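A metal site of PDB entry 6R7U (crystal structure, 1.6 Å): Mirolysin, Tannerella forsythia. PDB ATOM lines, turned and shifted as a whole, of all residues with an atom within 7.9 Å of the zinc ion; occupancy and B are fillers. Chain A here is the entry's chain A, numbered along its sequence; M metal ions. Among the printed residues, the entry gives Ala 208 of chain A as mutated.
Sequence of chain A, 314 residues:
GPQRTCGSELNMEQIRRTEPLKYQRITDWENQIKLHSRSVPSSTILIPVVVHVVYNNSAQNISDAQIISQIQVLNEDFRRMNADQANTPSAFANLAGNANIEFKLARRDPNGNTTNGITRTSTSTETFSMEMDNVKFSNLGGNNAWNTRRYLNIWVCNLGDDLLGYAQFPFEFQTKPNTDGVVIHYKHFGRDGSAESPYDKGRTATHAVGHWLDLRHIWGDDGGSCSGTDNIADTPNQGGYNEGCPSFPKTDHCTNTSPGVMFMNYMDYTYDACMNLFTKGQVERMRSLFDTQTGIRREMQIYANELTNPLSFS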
ATOM      1  N   ARG A   4     -21.287  27.896  -2.295  1.00  0.00           N
ATOM      2  CA  ARG A   4     -20.661  26.817  -1.529  1.00  0.00           C
ATOM      3  C   ARG A   4     -21.552  25.559  -1.484  1.00  0.00           C
ATOM      4  O   ARG A   4     -22.756  25.681  -1.221  1.00  0.00           O
ATOM      5  CB  ARG A   4     -20.351  27.272  -0.072  1.00  0.00           C
ATOM      6  CG  ARG A   4     -19.515  26.233   0.676  1.00  0.00           C
ATOM      7  CD  ARG A   4     -19.297  26.441   2.149  1.00  0.00           C
ATOM      8  NE  ARG A   4     -18.404  27.558   2.500  1.00  0.00           N
ATOM      9  CZ  ARG A   4     -17.076  27.510   2.507  1.00  0.00           C
ATOM     10  NH1 ARG A   4     -16.437  26.435   2.045  1.00  0.00           N
ATOM     11  NH2 ARG A   4     -16.369  28.545   2.909  1.00  0.00           N
ATOM     12  N   THR A   5     -20.966  24.372  -1.735  1.00  0.00           N
ATOM     13  CA  THR A   5     -21.695  23.100  -1.656  1.00  0.00           C
ATOM     14  C   THR A   5     -20.859  22.052  -0.904  1.00  0.00           C
ATOM     15  O   THR A   5     -19.659  21.900  -1.132  1.00  0.00           O
ATOM     16  CB  THR A   5     -22.139  22.578  -3.016  1.00  0.00           C
ATOM     17  OG1 THR A   5     -22.309  23.650  -3.939  1.00  0.00           O
ATOM     18  CG2 THR A   5     -23.424  21.731  -2.928  1.00  0.00           C
ATOM     19  N   CSX A   6     -21.516  21.329   0.002  1.00  0.00           N
ATOM     20  CA  CSX A   6     -20.888  20.308   0.839  1.00  0.00           C
ATOM     21  CB  CSX A   6     -20.874  21.056   2.171  1.00  0.00           C
ATOM     22  SG  CSX A   6     -20.654  19.908   3.525  1.00  0.00           S
ATOM     23  C   CSX A   6     -21.844  19.124   0.793  1.00  0.00           C
ATOM     24  O   CSX A   6     -23.055  19.305   0.637  1.00  0.00           O
ATOM     25  OD  CSX A   6     -19.217  19.669   3.427  1.00  0.00           O
ATOM     26  N   GLY A   7     -21.308  17.929   0.861  1.00  0.00           N
ATOM     27  CA  GLY A   7     -22.192  16.772   0.807  1.00  0.00           C
ATOM     28  C   GLY A   7     -22.509  16.196   2.166  1.00  0.00           C
ATOM     29  O   GLY A   7     -22.861  15.012   2.253  1.00  0.00           O
ATOM     30  N   SER A   8     -22.443  17.029   3.242  1.00  0.00           N
ATOM     31  CA  SER A   8     -22.648  16.440   4.546  1.00  0.00           C
ATOM     32  C   SER A   8     -23.861  17.033   5.244  1.00  0.00           C
ATOM     33  O   SER A   8     -23.768  17.671   6.287  1.00  0.00           O
ATOM     34  CB  SER A   8     -21.377  16.563   5.383  1.00  0.00           C
ATOM     35  OG  SER A   8     -20.418  15.720   4.765  1.00  0.00           O
ATOM     36  N   GLU A   9     -25.020  16.824   4.615  1.00  0.00           N
ATOM     37  CA  GLU A   9     -26.283  17.262   5.181  1.00  0.00           C
ATOM     38  C   GLU A   9     -26.849  16.171   6.050  1.00  0.00           C
ATOM     39  O   GLU A   9     -26.609  14.979   5.846  1.00  0.00           O
ATOM     40  CB  GLU A   9     -27.313  17.636   4.092  1.00  0.00           C
ATOM     41  CG  GLU A   9     -26.796  18.103   2.741  1.00  0.00           C
ATOM     42  CD  GLU A   9     -26.082  19.439   2.718  1.00  0.00           C
ATOM     43  OE1 GLU A   9     -26.757  20.483   2.633  1.00  0.00           O
ATOM     44  OE2 GLU A   9     -24.831  19.427   2.758  1.00  0.00           O
ATOM     45  N   GLY A 165     -16.437  19.820  -0.875  1.00  0.00           N
ATOM     46  CA  GLY A 165     -15.918  18.808   0.034  1.00  0.00           C
ATOM     47  C   GLY A 165     -17.029  18.042   0.701  1.00  0.00           C
ATOM     48  O   GLY A 165     -18.206  18.400   0.566  1.00  0.00           O
ATOM     49  N   TYR A 166     -16.665  17.021   1.459  1.00  0.00           N
ATOM     50  CA  TYR A 166     -17.667  16.317   2.273  1.00  0.00           C
ATOM     51  C   TYR A 166     -16.967  15.551   3.401  1.00  0.00           C
ATOM     52  O   TYR A 166     -15.801  15.208   3.287  1.00  0.00           O
ATOM     53  CB  TYR A 166     -18.545  15.372   1.436  1.00  0.00           C
ATOM     54  CG  TYR A 166     -17.830  14.172   0.844  1.00  0.00           C
ATOM     55  CD1 TYR A 166     -17.857  12.940   1.489  1.00  0.00           C
ATOM     56  CD2 TYR A 166     -17.262  14.243  -0.419  1.00  0.00           C
ATOM     57  CE1 TYR A 166     -17.299  11.803   0.912  1.00  0.00           C
ATOM     58  CE2 TYR A 166     -16.702  13.108  -1.021  1.00  0.00           C
ATOM     59  CZ  TYR A 166     -16.723  11.895  -0.353  1.00  0.00           C
ATOM     60  OH  TYR A 166     -16.179  10.778  -0.934  1.00  0.00           O
ATOM     61  N   ALA A 167     -17.673  15.289   4.455  1.00  0.00           N
ATOM     62  CA  ALA A 167     -17.080  14.613   5.586  1.00  0.00           C
ATOM     63  C   ALA A 167     -17.970  13.458   5.969  1.00  0.00           C
ATOM     64  O   ALA A 167     -19.144  13.413   5.551  1.00  0.00           O
ATOM     65  CB  ALA A 167     -17.013  15.609   6.757  1.00  0.00           C
ATOM     66  N   PHE A 169     -19.741  11.769   9.337  1.00  0.00           N
ATOM     67  CA  PHE A 169     -19.991  12.127  10.718  1.00  0.00           C
ATOM     68  C   PHE A 169     -19.558  11.060  11.702  1.00  0.00           C
ATOM     69  O   PHE A 169     -19.641   9.856  11.383  1.00  0.00           O
ATOM     70  CB  PHE A 169     -21.512  12.325  10.901  1.00  0.00           C
ATOM     71  CG  PHE A 169     -22.003  13.588  10.240  1.00  0.00           C
ATOM     72  CD1 PHE A 169     -22.603  13.536   8.984  1.00  0.00           C
ATOM     73  CD2 PHE A 169     -21.922  14.807  10.890  1.00  0.00           C
ATOM     74  CE1 PHE A 169     -23.078  14.714   8.382  1.00  0.00           C
ATOM     75  CE2 PHE A 169     -22.417  15.980  10.301  1.00  0.00           C
ATOM     76  CZ  PHE A 169     -22.995  15.929   9.049  1.00  0.00           C
ATOM     77  N   THR A 204     -12.936  25.503   3.581  1.00  0.00           N
ATOM     78  CA  THR A 204     -13.706  24.339   3.170  1.00  0.00           C
ATOM     79  C   THR A 204     -13.294  23.164   4.090  1.00  0.00           C
ATOM     80  O   THR A 204     -14.143  22.458   4.653  1.00  0.00           O
ATOM     81  CB  THR A 204     -13.441  23.964   1.716  1.00  0.00           C
ATOM     82  OG1 THR A 204     -13.886  25.036   0.916  1.00  0.00           O
ATOM     83  CG2 THR A 204     -14.186  22.713   1.331  1.00  0.00           C
ATOM     84  N   HIS A 207     -14.604  23.745   7.781  1.00  0.00           N
ATOM     85  CA  HIS A 207     -16.008  23.369   7.806  1.00  0.00           C
ATOM     86  C   HIS A 207     -16.109  21.835   7.772  1.00  0.00           C
ATOM     87  O   HIS A 207     -16.782  21.288   8.663  1.00  0.00           O
ATOM     88  CB  HIS A 207     -16.698  23.979   6.603  1.00  0.00           C
ATOM     89  CG  HIS A 207     -18.117  23.576   6.380  1.00  0.00           C
ATOM     90  ND1 HIS A 207     -19.169  24.482   6.526  1.00  0.00           N
ATOM     91  CD2 HIS A 207     -18.611  22.410   5.899  1.00  0.00           C
ATOM     92  CE1 HIS A 207     -20.239  23.837   6.108  1.00  0.00           C
ATOM     93  NE2 HIS A 207     -19.941  22.587   5.723  1.00  0.00           N
ATOM     94  N   ALA A 208     -15.423  21.172   6.844  1.00  0.00           N
ATOM     95  CA  ALA A 208     -15.539  19.700   6.775  1.00  0.00           C
ATOM     96  C   ALA A 208     -15.057  19.029   8.056  1.00  0.00           C
ATOM     97  O   ALA A 208     -15.654  18.073   8.538  1.00  0.00           O
ATOM     98  CB  ALA A 208     -14.775  19.125   5.570  1.00  0.00           C
ATOM     99  N   GLY A 210     -15.105  20.311  10.944  1.00  0.00           N
ATOM    100  CA  GLY A 210     -16.137  20.485  11.965  1.00  0.00           C
ATOM    101  C   GLY A 210     -17.164  19.340  11.904  1.00  0.00           C
ATOM    102  O   GLY A 210     -17.562  18.794  12.932  1.00  0.00           O
ATOM    103  N   HIS A 211     -17.587  18.916  10.665  1.00  0.00           N
ATOM    104  CA  HIS A 211     -18.535  17.770  10.519  1.00  0.00           C
ATOM    105  C   HIS A 211     -17.941  16.464  11.130  1.00  0.00           C
ATOM    106  O   HIS A 211     -18.583  15.710  11.837  1.00  0.00           O
ATOM    107  CB  HIS A 211     -18.883  17.463   9.054  1.00  0.00           C
ATOM    108  CG  HIS A 211     -19.774  18.480   8.417  1.00  0.00           C
ATOM    109  ND1 HIS A 211     -20.908  18.941   9.055  1.00  0.00           N
ATOM    110  CD2 HIS A 211     -19.716  19.028   7.164  1.00  0.00           C
ATOM    111  CE1 HIS A 211     -21.507  19.751   8.167  1.00  0.00           C
ATOM    112  NE2 HIS A 211     -20.786  19.884   7.057  1.00  0.00           N
ATOM    113  N   LEU A 215     -20.124  18.376  14.165  1.00  0.00           N
ATOM    114  CA  LEU A 215     -20.974  19.530  13.959  1.00  0.00           C
ATOM    115  C   LEU A 215     -21.871  19.362  12.712  1.00  0.00           C
ATOM    116  O   LEU A 215     -21.489  18.779  11.686  1.00  0.00           O
ATOM    117  CB  LEU A 215     -20.188  20.841  13.816  1.00  0.00           C
ATOM    118  CG  LEU A 215     -19.221  21.119  14.993  1.00  0.00           C
ATOM    119  CD1 LEU A 215     -18.520  22.451  14.844  1.00  0.00           C
ATOM    120  CD2 LEU A 215     -19.933  21.034  16.351  1.00  0.00           C
ATOM    121  N   ARG A 216     -23.025  19.980  12.792  1.00  0.00           N
ATOM    122  CA  ARG A 216     -23.945  20.039  11.637  1.00  0.00           C
ATOM    123  C   ARG A 216     -24.052  21.435  11.050  1.00  0.00           C
ATOM    124  O   ARG A 216     -23.740  22.415  11.704  1.00  0.00           O
ATOM    125  CB  ARG A 216     -25.373  19.651  12.091  1.00  0.00           C
ATOM    126  CG  ARG A 216     -25.456  18.230  12.625  1.00  0.00           C
ATOM    127  CD  ARG A 216     -26.912  18.014  12.991  1.00  0.00           C
ATOM    128  NE  ARG A 216     -27.095  16.722  13.636  1.00  0.00           N
ATOM    129  CZ  ARG A 216     -28.284  16.190  13.919  1.00  0.00           C
ATOM    130  NH1 ARG A 216     -29.398  16.835  13.614  1.00  0.00           N
ATOM    131  NH2 ARG A 216     -28.358  15.003  14.511  1.00  0.00           N
ATOM    132  N   HIS A 217     -24.605  21.550   9.816  1.00  0.00           N
ATOM    133  CA  HIS A 217     -24.830  22.860   9.216  1.00  0.00           C
ATOM    134  C   HIS A 217     -25.650  23.674  10.169  1.00  0.00           C
ATOM    135  O   HIS A 217     -26.659  23.190  10.683  1.00  0.00           O
ATOM    136  CB  HIS A 217     -25.593  22.661   7.924  1.00  0.00           C
ATOM    137  CG  HIS A 217     -24.661  22.106   6.901  1.00  0.00           C
ATOM    138  ND1 HIS A 217     -25.127  21.320   5.863  1.00  0.00           N
ATOM    139  CD2 HIS A 217     -23.314  22.204   6.813  1.00  0.00           C
ATOM    140  CE1 HIS A 217     -24.035  21.012   5.147  1.00  0.00           C
ATOM    141  NE2 HIS A 217     -22.928  21.538   5.678  1.00  0.00           N
ATOM    142  N   ILE A 218     -25.277  24.923  10.345  1.00  0.00           N
ATOM    143  CA  ILE A 218     -25.927  25.798  11.334  1.00  0.00           C
ATOM    144  C   ILE A 218     -27.440  26.003  11.076  1.00  0.00           C
ATOM    145  O   ILE A 218     -28.218  26.196  12.055  1.00  0.00           O
ATOM    146  CB  ILE A 218     -25.160  27.138  11.414  1.00  0.00           C
ATOM    147  CG1 ILE A 218     -25.670  28.006  12.508  1.00  0.00           C
ATOM    148  CG2 ILE A 218     -25.225  27.885  10.083  1.00  0.00           C
ATOM    149  CD1 ILE A 218     -24.677  29.178  12.872  1.00  0.00           C
ATOM    150  N   TRP A 219     -27.861  25.907   9.801  1.00  0.00           N
ATOM    151  CA  TRP A 219     -29.292  26.159   9.534  1.00  0.00           C
ATOM    152  C   TRP A 219     -30.183  24.906   9.707  1.00  0.00           C
ATOM    153  O   TRP A 219     -31.401  24.968   9.489  1.00  0.00           O
ATOM    154  CB  TRP A 219     -29.478  26.710   8.153  1.00  0.00           C
ATOM    155  CG  TRP A 219     -29.151  25.706   7.107  1.00  0.00           C
ATOM    156  CD1 TRP A 219     -30.032  24.983   6.350  1.00  0.00           C
ATOM    157  CD2 TRP A 219     -27.866  25.503   6.544  1.00  0.00           C
ATOM    158  NE1 TRP A 219     -29.339  24.235   5.421  1.00  0.00           N
ATOM    159  CE2 TRP A 219     -28.001  24.522   5.526  1.00  0.00           C
ATOM    160  CE3 TRP A 219     -26.613  26.098   6.753  1.00  0.00           C
ATOM    161  CZ2 TRP A 219     -26.915  24.115   4.741  1.00  0.00           C
ATOM    162  CZ3 TRP A 219     -25.524  25.634   6.017  1.00  0.00           C
ATOM    163  CH2 TRP A 219     -25.675  24.681   5.016  1.00  0.00           C
ATOM    164  N   ASP A 221     -30.201  21.939   7.912  1.00  0.00           N
ATOM    165  CA  ASP A 221     -30.445  21.081   6.727  1.00  0.00           C
ATOM    166  C   ASP A 221     -31.945  20.782   6.520  1.00  0.00           C
ATOM    167  O   ASP A 221     -32.381  19.645   6.293  1.00  0.00           O
ATOM    168  CB  ASP A 221     -29.632  19.809   6.899  1.00  0.00           C
ATOM    169  CG  ASP A 221     -28.148  20.051   6.777  1.00  0.00           C
ATOM    170  OD1 ASP A 221     -27.736  20.709   5.821  1.00  0.00           O
ATOM    171  OD2 ASP A 221     -27.407  19.575   7.653  1.00  0.00           O
ATOM    172  N   TYR A 266     -18.248  28.970  10.918  1.00  0.00           N
ATOM    173  CA  TYR A 266     -17.678  28.072   9.892  1.00  0.00           C
ATOM    174  C   TYR A 266     -18.660  27.080   9.322  1.00  0.00           C
ATOM    175  O   TYR A 266     -18.414  26.550   8.226  1.00  0.00           O
ATOM    176  CB  TYR A 266     -16.505  27.303  10.444  1.00  0.00           C
ATOM    177  CG  TYR A 266     -15.403  28.212  10.914  1.00  0.00           C
ATOM    178  CD1 TYR A 266     -14.820  29.127  10.060  1.00  0.00           C
ATOM    179  CD2 TYR A 266     -14.989  28.194  12.254  1.00  0.00           C
ATOM    180  CE1 TYR A 266     -13.769  29.926  10.457  1.00  0.00           C
ATOM    181  CE2 TYR A 266     -13.990  29.053  12.693  1.00  0.00           C
ATOM    182  CZ  TYR A 266     -13.352  29.891  11.780  1.00  0.00           C
ATOM    183  OH  TYR A 266     -12.377  30.762  12.196  1.00  0.00           O
ATOM    184  N   MET A 267     -19.723  26.726  10.097  1.00  0.00           N
ATOM    185  CA  MET A 267     -20.675  25.700   9.641  1.00  0.00           C
ATOM    186  C   MET A 267     -21.831  26.277   8.772  1.00  0.00           C
ATOM    187  O   MET A 267     -22.849  25.571   8.572  1.00  0.00           O
ATOM    188  CB  MET A 267     -21.226  24.897  10.800  1.00  0.00           C
ATOM    189  CG  MET A 267     -20.151  24.437  11.719  1.00  0.00           C
ATOM    190  SD  MET A 267     -18.805  23.333  10.630  1.00  0.00           S
ATOM    191  CE  MET A 267     -20.008  22.052   9.750  1.00  0.00           C
ATOM    192  N   ASP A 268     -21.687  27.563   8.283  1.00  0.00           N
ATOM    193  CA  ASP A 268     -22.595  28.097   7.289  1.00  0.00           C
ATOM    194  C   ASP A 268     -21.979  27.842   5.928  1.00  0.00           C
ATOM    195  O   ASP A 268     -21.048  27.021   5.828  1.00  0.00           O
ATOM    196  CB  ASP A 268     -22.890  29.587   7.517  1.00  0.00           C
ATOM    197  CG  ASP A 268     -24.303  29.993   7.059  1.00  0.00           C
ATOM    198  OD1 ASP A 268     -24.845  29.374   6.121  1.00  0.00           O
ATOM    199  OD2 ASP A 268     -24.876  30.923   7.653  1.00  0.00           O
ATOM    200  N   TYR A 269     -22.538  28.474   4.852  1.00  0.00           N
ATOM    201  CA  TYR A 269     -22.087  28.269   3.467  1.00  0.00           C
ATOM    202  C   TYR A 269     -21.536  29.568   2.870  1.00  0.00           C
ATOM    203  O   TYR A 269     -21.431  29.689   1.650  1.00  0.00           O
ATOM    204  CB  TYR A 269     -23.271  27.795   2.611  1.00  0.00           C
ATOM    205  CG  TYR A 269     -23.439  26.295   2.463  1.00  0.00           C
ATOM    206  CD1 TYR A 269     -22.646  25.404   3.174  1.00  0.00           C
ATOM    207  CD2 TYR A 269     -24.476  25.775   1.694  1.00  0.00           C
ATOM    208  CE1 TYR A 269     -22.777  24.023   3.006  1.00  0.00           C
ATOM    209  CE2 TYR A 269     -24.629  24.393   1.523  1.00  0.00           C
ATOM    210  CZ  TYR A 269     -23.772  23.515   2.186  1.00  0.00           C
ATOM    211  OH  TYR A 269     -24.001  22.155   2.068  1.00  0.00           O
HETATM  212 ZN    ZN M   1     -21.081  21.018   5.341  1.00  0.00          ZN
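A ring nitrogen (ND1) of His 217 is in hydrogen-bond range of the side-chain carboxylate (OD1) of Asp 221.
SG of CSX 6 sits close to the backbone NH (N) of Ser 8 (3.4 Å).
A ring nitrogen (ND1) of His 211 sits at hydrogen-bond distance from the backbone carbonyl oxygen (O) of Leu 215 (2.7 Å).
O of CSX 6 lies close to OH of Tyr 269 (3.3 Å).
A ring nitrogen (ND1) of His 207 sits at hydrogen-bond distance from the backbone carbonyl oxygen of Tyr 266 (2.8 Å).
A ring nitrogen (ND1) of His 207 lies within hydrogen-bond range of the backbone carbonyl oxygen (O) of Asp 268, 3.2 Å away.
The nearest printed residue that does not touch the zinc ion is Tyr 269 (4.2 Å).
The zinc ion is bound by a ring nitrogen (NE2) of His 217 (1.9 Å), a ring nitrogen (NE2) of His 207 (2.0 Å), a ring nitrogen (NE2) of His 211 (2.1 Å) and SG of CSX 6 (2.2 Å).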
